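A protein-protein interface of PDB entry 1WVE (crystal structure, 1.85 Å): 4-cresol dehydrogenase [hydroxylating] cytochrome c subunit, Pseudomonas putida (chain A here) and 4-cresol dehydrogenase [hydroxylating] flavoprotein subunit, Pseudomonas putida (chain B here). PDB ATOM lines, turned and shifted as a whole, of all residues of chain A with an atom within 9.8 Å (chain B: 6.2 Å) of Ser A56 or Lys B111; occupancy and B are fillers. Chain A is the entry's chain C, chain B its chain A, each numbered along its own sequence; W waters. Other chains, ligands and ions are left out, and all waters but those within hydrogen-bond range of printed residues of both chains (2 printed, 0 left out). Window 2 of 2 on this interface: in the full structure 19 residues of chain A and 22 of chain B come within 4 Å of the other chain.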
ATOM      1  N   GLN A   3     -33.062   0.247 -20.903  1.00  0.00           N
ATOM      2  CA  GLN A   3     -33.242   1.021 -19.680  1.00  0.00           C
ATOM      3  C   GLN A   3     -34.310   2.099 -19.848  1.00  0.00           C
ATOM      4  O   GLN A   3     -35.050   2.394 -18.917  1.00  0.00           O
ATOM      5  CB  GLN A   3     -31.920   1.660 -19.259  1.00  0.00           C
ATOM      6  CG  GLN A   3     -31.984   2.366 -17.915  1.00  0.00           C
ATOM      7  CD  GLN A   3     -30.704   3.097 -17.614  1.00  0.00           C
ATOM      8  OE1 GLN A   3     -30.237   3.898 -18.420  1.00  0.00           O
ATOM      9  NE2 GLN A   3     -30.125   2.833 -16.454  1.00  0.00           N
ATOM     10  N   TRP A   4     -34.385   2.691 -21.033  1.00  0.00           N
ATOM     11  CA  TRP A   4     -35.376   3.725 -21.290  1.00  0.00           C
ATOM     12  C   TRP A   4     -36.291   3.392 -22.468  1.00  0.00           C
ATOM     13  O   TRP A   4     -37.180   4.171 -22.802  1.00  0.00           O
ATOM     14  CB  TRP A   4     -34.688   5.075 -21.516  1.00  0.00           C
ATOM     15  CG  TRP A   4     -34.072   5.623 -20.255  1.00  0.00           C
ATOM     16  CD1 TRP A   4     -32.776   5.477 -19.839  1.00  0.00           C
ATOM     17  CD2 TRP A   4     -34.750   6.342 -19.217  1.00  0.00           C
ATOM     18  NE1 TRP A   4     -32.606   6.066 -18.600  1.00  0.00           N
ATOM     19  CE2 TRP A   4     -33.802   6.601 -18.196  1.00  0.00           C
ATOM     20  CE3 TRP A   4     -36.066   6.792 -19.047  1.00  0.00           C
ATOM     21  CZ2 TRP A   4     -34.130   7.293 -17.021  1.00  0.00           C
ATOM     22  CZ3 TRP A   4     -36.392   7.479 -17.878  1.00  0.00           C
ATOM     23  CH2 TRP A   4     -35.426   7.721 -16.880  1.00  0.00           C
ATOM     24  N   LEU A  10     -36.260   8.624 -23.328  1.00  0.00           N
ATOM     25  CA  LEU A  10     -35.266   9.187 -22.410  1.00  0.00           C
ATOM     26  C   LEU A  10     -35.370  10.707 -22.469  1.00  0.00           C
ATOM     27  O   LEU A  10     -35.360  11.390 -21.441  1.00  0.00           O
ATOM     28  CB  LEU A  10     -33.844   8.776 -22.803  1.00  0.00           C
ATOM     29  CG  LEU A  10     -32.754   9.533 -22.021  1.00  0.00           C
ATOM     30  CD1 LEU A  10     -32.891   9.212 -20.526  1.00  0.00           C
ATOM     31  CD2 LEU A  10     -31.369   9.131 -22.530  1.00  0.00           C
ATOM     32  N   VAL A  43     -23.043  14.193 -20.604  1.00  0.00           N
ATOM     33  CA  VAL A  43     -23.883  13.521 -19.617  1.00  0.00           C
ATOM     34  C   VAL A  43     -23.063  12.864 -18.501  1.00  0.00           C
ATOM     35  O   VAL A  43     -23.435  12.956 -17.334  1.00  0.00           O
ATOM     36  CB  VAL A  43     -24.788  12.464 -20.293  1.00  0.00           C
ATOM     37  CG1 VAL A  43     -25.586  11.686 -19.243  1.00  0.00           C
ATOM     38  CG2 VAL A  43     -25.763  13.168 -21.246  1.00  0.00           C
ATOM     39  N   ARG A  44     -21.950  12.223 -18.851  1.00  0.00           N
ATOM     40  CA  ARG A  44     -21.119  11.557 -17.846  1.00  0.00           C
ATOM     41  C   ARG A  44     -20.336  12.507 -16.950  1.00  0.00           C
ATOM     42  O   ARG A  44     -20.165  12.248 -15.760  1.00  0.00           O
ATOM     43  CB  ARG A  44     -20.138  10.597 -18.514  1.00  0.00           C
ATOM     44  CG  ARG A  44     -20.796   9.377 -19.132  1.00  0.00           C
ATOM     45  CD  ARG A  44     -21.378   8.438 -18.063  1.00  0.00           C
ATOM     46  NE  ARG A  44     -22.024   7.301 -18.705  1.00  0.00           N
ATOM     47  CZ  ARG A  44     -23.330   7.070 -18.695  1.00  0.00           C
ATOM     48  NH1 ARG A  44     -24.160   7.895 -18.051  1.00  0.00           N
ATOM     49  NH2 ARG A  44     -23.803   6.033 -19.367  1.00  0.00           N
ATOM     50  N   ALA A  52     -24.531  15.755 -13.845  1.00  0.00           N
ATOM     51  CA  ALA A  52     -24.009  14.561 -14.498  1.00  0.00           C
ATOM     52  C   ALA A  52     -24.964  13.433 -14.150  1.00  0.00           C
ATOM     53  O   ALA A  52     -25.686  13.516 -13.156  1.00  0.00           O
ATOM     54  CB  ALA A  52     -22.631  14.237 -13.983  1.00  0.00           C
ATOM     55  N   PHE A  53     -24.976  12.389 -14.971  1.00  0.00           N
ATOM     56  CA  PHE A  53     -25.816  11.236 -14.717  1.00  0.00           C
ATOM     57  C   PHE A  53     -24.984   9.964 -14.780  1.00  0.00           C
ATOM     58  O   PHE A  53     -24.322   9.696 -15.786  1.00  0.00           O
ATOM     59  CB  PHE A  53     -26.952  11.114 -15.751  1.00  0.00           C
ATOM     60  CG  PHE A  53     -28.039  12.137 -15.588  1.00  0.00           C
ATOM     61  CD1 PHE A  53     -27.903  13.412 -16.142  1.00  0.00           C
ATOM     62  CD2 PHE A  53     -29.177  11.843 -14.832  1.00  0.00           C
ATOM     63  CE1 PHE A  53     -28.885  14.387 -15.940  1.00  0.00           C
ATOM     64  CE2 PHE A  53     -30.169  12.813 -14.625  1.00  0.00           C
ATOM     65  CZ  PHE A  53     -30.021  14.088 -15.179  1.00  0.00           C
ATOM     66  N   PRO A  54     -24.983   9.174 -13.698  1.00  0.00           N
ATOM     67  CA  PRO A  54     -24.218   7.923 -13.702  1.00  0.00           C
ATOM     68  C   PRO A  54     -24.896   6.950 -14.678  1.00  0.00           C
ATOM     69  O   PRO A  54     -26.069   7.125 -15.018  1.00  0.00           O
ATOM     70  CB  PRO A  54     -24.346   7.431 -12.262  1.00  0.00           C
ATOM     71  CG  PRO A  54     -24.502   8.706 -11.479  1.00  0.00           C
ATOM     72  CD  PRO A  54     -25.473   9.486 -12.342  1.00  0.00           C
ATOM     73  N   ALA A  55     -24.160   5.933 -15.115  1.00  0.00           N
ATOM     74  CA  ALA A  55     -24.687   4.918 -16.020  1.00  0.00           C
ATOM     75  C   ALA A  55     -25.880   4.178 -15.375  1.00  0.00           C
ATOM     76  O   ALA A  55     -26.745   3.648 -16.080  1.00  0.00           O
ATOM     77  CB  ALA A  55     -23.563   3.916 -16.391  1.00  0.00           C
ATOM     78  N   SER A  56     -25.935   4.144 -14.042  1.00  0.00           N
ATOM     79  CA  SER A  56     -27.045   3.474 -13.353  1.00  0.00           C
ATOM     80  C   SER A  56     -28.349   4.229 -13.592  1.00  0.00           C
ATOM     81  O   SER A  56     -29.437   3.662 -13.488  1.00  0.00           O
ATOM     82  CB  SER A  56     -26.777   3.383 -11.842  1.00  0.00           C
ATOM     83  OG  SER A  56     -26.690   4.678 -11.277  1.00  0.00           O
ATOM     84  N   TYR A  57     -28.236   5.514 -13.918  1.00  0.00           N
ATOM     85  CA  TYR A  57     -29.417   6.344 -14.183  1.00  0.00           C
ATOM     86  C   TYR A  57     -29.700   6.382 -15.691  1.00  0.00           C
ATOM     87  O   TYR A  57     -30.841   6.222 -16.127  1.00  0.00           O
ATOM     88  CB  TYR A  57     -29.183   7.768 -13.667  1.00  0.00           C
ATOM     89  CG  TYR A  57     -30.452   8.523 -13.315  1.00  0.00           C
ATOM     90  CD1 TYR A  57     -31.449   8.742 -14.265  1.00  0.00           C
ATOM     91  CD2 TYR A  57     -30.657   9.008 -12.021  1.00  0.00           C
ATOM     92  CE1 TYR A  57     -32.622   9.426 -13.935  1.00  0.00           C
ATOM     93  CE2 TYR A  57     -31.831   9.691 -11.678  1.00  0.00           C
ATOM     94  CZ  TYR A  57     -32.803   9.895 -12.637  1.00  0.00           C
ATOM     95  OH  TYR A  57     -33.957  10.565 -12.301  1.00  0.00           O
ATOM     96  N   VAL A  58     -28.652   6.582 -16.485  1.00  0.00           N
ATOM     97  CA  VAL A  58     -28.779   6.635 -17.944  1.00  0.00           C
ATOM     98  C   VAL A  58     -27.593   5.887 -18.546  1.00  0.00           C
ATOM     99  O   VAL A  58     -26.478   6.414 -18.588  1.00  0.00           O
ATOM    100  CB  VAL A  58     -28.764   8.095 -18.459  1.00  0.00           C
ATOM    101  CG1 VAL A  58     -28.991   8.119 -19.964  1.00  0.00           C
ATOM    102  CG2 VAL A  58     -29.825   8.907 -17.760  1.00  0.00           C
ATOM    103  N   ASP A  59     -27.828   4.663 -19.016  1.00  0.00           N
ATOM    104  CA  ASP A  59     -26.739   3.860 -19.569  1.00  0.00           C
ATOM    105  C   ASP A  59     -26.266   4.268 -20.966  1.00  0.00           C
ATOM    106  O   ASP A  59     -26.894   5.094 -21.635  1.00  0.00           O
ATOM    107  CB  ASP A  59     -27.099   2.363 -19.551  1.00  0.00           C
ATOM    108  CG  ASP A  59     -28.308   2.022 -20.409  1.00  0.00           C
ATOM    109  OD1 ASP A  59     -28.713   2.819 -21.290  1.00  0.00           O
ATOM    110  OD2 ASP A  59     -28.853   0.920 -20.204  1.00  0.00           O
ATOM    111  N   ASP A  60     -25.141   3.698 -21.384  1.00  0.00           N
ATOM    112  CA  ASP A  60     -24.558   4.001 -22.690  1.00  0.00           C
ATOM    113  C   ASP A  60     -25.499   3.763 -23.855  1.00  0.00           C
ATOM    114  O   ASP A  60     -25.559   4.567 -24.782  1.00  0.00           O
ATOM    115  CB  ASP A  60     -23.275   3.190 -22.915  1.00  0.00           C
ATOM    116  CG  ASP A  60     -22.131   3.639 -22.011  1.00  0.00           C
ATOM    117  OD1 ASP A  60     -22.303   4.633 -21.266  1.00  0.00           O
ATOM    118  OD2 ASP A  60     -21.056   2.997 -22.049  1.00  0.00           O
ATOM    119  N   SER A  62     -28.728   3.918 -23.951  1.00  0.00           N
ATOM    120  CA  SER A  62     -29.730   4.978 -23.986  1.00  0.00           C
ATOM    121  C   SER A  62     -29.154   6.288 -24.529  1.00  0.00           C
ATOM    122  O   SER A  62     -29.866   7.067 -25.176  1.00  0.00           O
ATOM    123  CB  SER A  62     -30.316   5.205 -22.587  1.00  0.00           C
ATOM    124  OG  SER A  62     -30.967   4.035 -22.128  1.00  0.00           O
ATOM    125  N   LEU A  63     -27.876   6.543 -24.264  1.00  0.00           N
ATOM    126  CA  LEU A  63     -27.235   7.756 -24.766  1.00  0.00           C
ATOM    127  C   LEU A  63     -27.079   7.627 -26.293  1.00  0.00           C
ATOM    128  O   LEU A  63     -27.252   8.598 -27.028  1.00  0.00           O
ATOM    129  CB  LEU A  63     -25.879   7.951 -24.091  1.00  0.00           C
ATOM    130  CG  LEU A  63     -25.803   8.921 -22.892  1.00  0.00           C
ATOM    131  CD1 LEU A  63     -27.160   9.198 -22.326  1.00  0.00           C
ATOM    132  CD2 LEU A  63     -24.878   8.355 -21.840  1.00  0.00           C
ATOM    133  N   ASP B  31     -20.163  -6.027 -13.447  1.00  0.00           N
ATOM    134  CA  ASP B  31     -20.886  -4.889 -13.992  1.00  0.00           C
ATOM    135  C   ASP B  31     -21.479  -3.985 -12.905  1.00  0.00           C
ATOM    136  O   ASP B  31     -21.854  -2.843 -13.179  1.00  0.00           O
ATOM    137  CB  ASP B  31     -21.998  -5.391 -14.918  1.00  0.00           C
ATOM    138  CG  ASP B  31     -21.455  -6.047 -16.199  1.00  0.00           C
ATOM    139  OD1 ASP B  31     -22.240  -6.741 -16.880  1.00  0.00           O
ATOM    140  OD2 ASP B  31     -20.254  -5.867 -16.531  1.00  0.00           O
ATOM    141  N   ASN B  32     -21.549  -4.493 -11.681  1.00  0.00           N
ATOM    142  CA  ASN B  32     -22.104  -3.722 -10.577  1.00  0.00           C
ATOM    143  C   ASN B  32     -21.061  -3.183  -9.615  1.00  0.00           C
ATOM    144  O   ASN B  32     -21.385  -2.692  -8.531  1.00  0.00           O
ATOM    145  CB  ASN B  32     -23.134  -4.576  -9.841  1.00  0.00           C
ATOM    146  CG  ASN B  32     -24.377  -4.798 -10.678  1.00  0.00           C
ATOM    147  OD1 ASN B  32     -25.099  -3.848 -10.983  1.00  0.00           O
ATOM    148  ND2 ASN B  32     -24.620  -6.040 -11.076  1.00  0.00           N
ATOM    149  N   TYR B  43     -20.485  10.576 -10.647  1.00  0.00           N
ATOM    150  CA  TYR B  43     -20.849  10.666  -9.226  1.00  0.00           C
ATOM    151  C   TYR B  43     -20.113  11.837  -8.550  1.00  0.00           C
ATOM    152  O   TYR B  43     -20.512  12.315  -7.476  1.00  0.00           O
ATOM    153  CB  TYR B  43     -20.437   9.387  -8.489  1.00  0.00           C
ATOM    154  CG  TYR B  43     -21.155   8.122  -8.894  1.00  0.00           C
ATOM    155  CD1 TYR B  43     -22.418   7.822  -8.392  1.00  0.00           C
ATOM    156  CD2 TYR B  43     -20.549   7.199  -9.756  1.00  0.00           C
ATOM    157  CE1 TYR B  43     -23.066   6.632  -8.734  1.00  0.00           C
ATOM    158  CE2 TYR B  43     -21.179   6.013 -10.100  1.00  0.00           C
ATOM    159  CZ  TYR B  43     -22.437   5.733  -9.586  1.00  0.00           C
ATOM    160  OH  TYR B  43     -23.062   4.555  -9.921  1.00  0.00           O
ATOM    161  N   THR B  62     -23.507  -0.979  -7.294  1.00  0.00           N
ATOM    162  CA  THR B  62     -24.945  -0.868  -7.489  1.00  0.00           C
ATOM    163  C   THR B  62     -25.650  -2.142  -7.055  1.00  0.00           C
ATOM    164  O   THR B  62     -25.350  -3.227  -7.558  1.00  0.00           O
ATOM    165  CB  THR B  62     -25.265  -0.574  -8.972  1.00  0.00           C
ATOM    166  OG1 THR B  62     -24.530  -1.476  -9.810  1.00  0.00           O
ATOM    167  CG2 THR B  62     -24.874   0.846  -9.322  1.00  0.00           C
ATOM    168  N   ALA B  63     -26.583  -2.019  -6.113  1.00  0.00           N
ATOM    169  CA  ALA B  63     -27.319  -3.175  -5.626  1.00  0.00           C
ATOM    170  C   ALA B  63     -28.779  -3.067  -6.031  1.00  0.00           C
ATOM    171  O   ALA B  63     -29.304  -1.953  -6.191  1.00  0.00           O
ATOM    172  CB  ALA B  63     -27.199  -3.271  -4.096  1.00  0.00           C
ATOM    173  N   THR B  64     -29.440  -4.211  -6.209  1.00  0.00           N
ATOM    174  CA  THR B  64     -30.845  -4.199  -6.592  1.00  0.00           C
ATOM    175  C   THR B  64     -31.726  -4.959  -5.613  1.00  0.00           C
ATOM    176  O   THR B  64     -32.945  -4.953  -5.752  1.00  0.00           O
ATOM    177  CB  THR B  64     -31.054  -4.825  -7.980  1.00  0.00           C
ATOM    178  OG1 THR B  64     -30.474  -6.130  -7.987  1.00  0.00           O
ATOM    179  CG2 THR B  64     -30.396  -3.970  -9.049  1.00  0.00           C
ATOM    180  N   SER B  87     -29.761   7.228  -3.249  1.00  0.00           N
ATOM    181  CA  SER B  87     -30.911   6.560  -3.853  1.00  0.00           C
ATOM    182  C   SER B  87     -30.997   7.042  -5.304  1.00  0.00           C
ATOM    183  O   SER B  87     -30.596   6.317  -6.215  1.00  0.00           O
ATOM    184  CB  SER B  87     -32.175   6.905  -3.069  1.00  0.00           C
ATOM    185  OG  SER B  87     -32.092   6.371  -1.760  1.00  0.00           O
ATOM    186  N   ASP B 108     -24.757   2.844  -4.537  1.00  0.00           N
ATOM    187  CA  ASP B 108     -25.722   3.467  -5.429  1.00  0.00           C
ATOM    188  C   ASP B 108     -26.949   2.562  -5.610  1.00  0.00           C
ATOM    189  O   ASP B 108     -26.876   1.521  -6.263  1.00  0.00           O
ATOM    190  CB  ASP B 108     -25.016   3.739  -6.764  1.00  0.00           C
ATOM    191  CG  ASP B 108     -25.937   4.302  -7.828  1.00  0.00           C
ATOM    192  OD1 ASP B 108     -25.480   4.433  -8.990  1.00  0.00           O
ATOM    193  OD2 ASP B 108     -27.102   4.613  -7.511  1.00  0.00           O
ATOM    194  N   LEU B 109     -28.077   2.967  -5.029  1.00  0.00           N
ATOM    195  CA  LEU B 109     -29.310   2.182  -5.107  1.00  0.00           C
ATOM    196  C   LEU B 109     -30.277   2.578  -6.228  1.00  0.00           C
ATOM    197  O   LEU B 109     -31.442   2.180  -6.218  1.00  0.00           O
ATOM    198  CB  LEU B 109     -30.037   2.243  -3.747  1.00  0.00           C
ATOM    199  CG  LEU B 109     -29.186   1.770  -2.546  1.00  0.00           C
ATOM    200  CD1 LEU B 109     -29.991   1.865  -1.222  1.00  0.00           C
ATOM    201  CD2 LEU B 109     -28.757   0.329  -2.787  1.00  0.00           C
ATOM    202  N   LYS B 110     -29.801   3.347  -7.203  1.00  0.00           N
ATOM    203  CA  LYS B 110     -30.663   3.791  -8.292  1.00  0.00           C
ATOM    204  C   LYS B 110     -31.369   2.663  -9.051  1.00  0.00           C
ATOM    205  O   LYS B 110     -32.501   2.844  -9.520  1.00  0.00           O
ATOM    206  CB  LYS B 110     -29.868   4.649  -9.289  1.00  0.00           C
ATOM    207  CG  LYS B 110     -30.704   5.177 -10.464  1.00  0.00           C
ATOM    208  CD  LYS B 110     -31.749   6.197  -9.998  1.00  0.00           C
ATOM    209  CE  LYS B 110     -32.830   6.453 -11.048  1.00  0.00           C
ATOM    210  NZ  LYS B 110     -33.764   5.295 -11.178  1.00  0.00           N
ATOM    211  N   LYS B 111     -30.715   1.513  -9.185  1.00  0.00           N
ATOM    212  CA  LYS B 111     -31.317   0.387  -9.911  1.00  0.00           C
ATOM    213  C   LYS B 111     -32.329  -0.418  -9.080  1.00  0.00           C
ATOM    214  O   LYS B 111     -33.071  -1.248  -9.613  1.00  0.00           O
ATOM    215  CB  LYS B 111     -30.209  -0.517 -10.477  1.00  0.00           C
ATOM    216  CG  LYS B 111     -29.318   0.233 -11.473  1.00  0.00           C
ATOM    217  CD  LYS B 111     -28.538  -0.706 -12.385  1.00  0.00           C
ATOM    218  CE  LYS B 111     -27.730  -1.732 -11.609  1.00  0.00           C
ATOM    219  NZ  LYS B 111     -27.132  -2.767 -12.516  1.00  0.00           N
ATOM    220  N   MET B 112     -32.349  -0.170  -7.772  1.00  0.00           N
ATOM    221  CA  MET B 112     -33.283  -0.835  -6.863  1.00  0.00           C
ATOM    222  C   MET B 112     -34.501   0.075  -6.952  1.00  0.00           C
ATOM    223  O   MET B 112     -34.821   0.824  -6.026  1.00  0.00           O
ATOM    224  CB  MET B 112     -32.692  -0.862  -5.441  1.00  0.00           C
ATOM    225  CG  MET B 112     -33.525  -1.582  -4.384  1.00  0.00           C
ATOM    226  SD  MET B 112     -32.608  -1.791  -2.823  1.00  0.00           S
ATOM    227  CE  MET B 112     -33.366  -3.175  -2.184  1.00  0.00           C
ATOM    228  N   ASN B 113     -35.174   0.002  -8.096  1.00  0.00           N
ATOM    229  CA  ASN B 113     -36.306   0.867  -8.396  1.00  0.00           C
ATOM    230  C   ASN B 113     -37.723   0.341  -8.557  1.00  0.00           C
ATOM    231  O   ASN B 113     -38.466   0.819  -9.432  1.00  0.00           O
ATOM    232  CB  ASN B 113     -35.959   1.673  -9.662  1.00  0.00           C
ATOM    233  CG  ASN B 113     -35.889   0.794 -10.923  1.00  0.00           C
ATOM    234  OD1 ASN B 113     -35.840   1.302 -12.049  1.00  0.00           O
ATOM    235  ND2 ASN B 113     -35.881  -0.516 -10.738  1.00  0.00           N
ATOM    236  N   LYS B 114     -38.135  -0.584  -7.703  1.00  0.00           N
ATOM    237  CA  LYS B 114     -39.489  -1.103  -7.816  1.00  0.00           C
ATOM    238  C   LYS B 114     -40.500  -0.300  -7.026  1.00  0.00           C
ATOM    239  O   LYS B 114     -40.250   0.102  -5.887  1.00  0.00           O
ATOM    240  CB  LYS B 114     -39.568  -2.549  -7.330  1.00  0.00           C
ATOM    241  CG  LYS B 114     -38.758  -3.532  -8.157  1.00  0.00           C
ATOM    242  CD  LYS B 114     -38.864  -4.947  -7.573  1.00  0.00           C
ATOM    243  CE  LYS B 114     -37.916  -5.902  -8.280  1.00  0.00           C
ATOM    244  NZ  LYS B 114     -37.991  -7.271  -7.714  1.00  0.00           N
ATOM    245  N   GLU B 128     -39.029   1.484  -3.445  1.00  0.00           N
ATOM    246  CA  GLU B 128     -37.619   1.224  -3.261  1.00  0.00           C
ATOM    247  C   GLU B 128     -36.872   2.536  -3.525  1.00  0.00           C
ATOM    248  O   GLU B 128     -37.406   3.459  -4.129  1.00  0.00           O
ATOM    249  CB  GLU B 128     -37.158   0.121  -4.214  1.00  0.00           C
ATOM    250  CG  GLU B 128     -37.760  -1.233  -3.872  1.00  0.00           C
ATOM    251  CD  GLU B 128     -37.062  -2.375  -4.578  1.00  0.00           C
ATOM    252  OE1 GLU B 128     -36.670  -2.182  -5.748  1.00  0.00           O
ATOM    253  OE2 GLU B 128     -36.918  -3.461  -3.960  1.00  0.00           O
ATOM    254  N   GLY B 130     -34.473   3.615  -5.684  1.00  0.00           N
ATOM    255  CA  GLY B 130     -34.273   4.117  -7.037  1.00  0.00           C
ATOM    256  C   GLY B 130     -35.517   4.641  -7.743  1.00  0.00           C
ATOM    257  O   GLY B 130     -35.428   5.156  -8.870  1.00  0.00           O
HETATM  258  O   HOH W   1     -23.331   4.084 -12.570  1.00  0.00           O
HETATM  259  O   HOH W   2     -32.252   3.296 -12.917  1.00  0.00           O
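OD1 of Asp B108 sits at hydrogen-bond distance from OG of Ser A56, 2.6 Å away.
Among the printed residues, merely in contact across the chains: Pro A54 with Tyr B43 (3.7 Å), Ser A56 with Tyr B43 (3.9 Å), Ser A56 with Lys B110 (3.6 Å), Ser A56 with Lys B111 (3.98 Å) and Tyr A57 with Lys B110 (3.4 Å).
Water W1 lies within hydrogen-bond range of OH of Tyr B43 (2.7 Å), N of Ser A56 (3.0 Å) and N of Ala A55 (3.3 Å).
Water W2 lies within hydrogen-bond range of the backbone carbonyl oxygen (O) of Ser A56 (2.9 Å) and the side-chain amino group (NZ) of Lys B110 (3.1 Å).
Trp A4 touches none of the printed residues of chain B.
Ser A56 touches just these residues of chain B: Tyr B43 (3.9 Å), Asp B108 (2.6 Å), Lys B110 (3.6 Å) and Lys B111 (3.98 Å).
Printed residues of chain A within 4 Å of Tyr B43: Pro A54 (3.7 Å) and Ser A56 (3.9 Å).
Printed residues of chain A within 4 Å of Asp B108: Ser A56 (2.6 Å).
Lys B111 touches one residue of chain A.
The nearest residue of chain B that does not touch Ser A56 is Thr B62 (4.1 Å).
The side-chain amide oxygen (OD1) of Asn B32 sits at hydrogen-bond distance from the side-chain amino group (NZ) of Lys B111.
The backbone carbonyl oxygen (O) of Tyr A57 lies within hydrogen-bond range of the indole nitrogen (NE1) of Trp A4.
OD2 of Asp B108 sits at hydrogen-bond distance from N of Lys B110 (3.0 Å).
The backbone carbonyl oxygen (O) of Gly B130 lies within hydrogen-bond range of the side-chain amino group (NZ) of Lys B110 (2.8 Å).
O of Ser B87 is in hydrogen-bond range of N of Lys B110, at 3.2 Å.
The side-chain amide nitrogen of Gln A3 is in hydrogen-bond range of the backbone carbonyl oxygen of Ser A56, 3.2 Å away.
Hydrophobic or aromatic side chains of chain A within 4 Å of the printed part of chain B: Pro A54 and Tyr A57.
Of the 16 printed residues of chain B, 4 touch a printed residue of chain A.
Printed residues of chain B that touch a printed residue of chain A: Tyr B43, Asp B108, Lys B110 and Lys B111.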
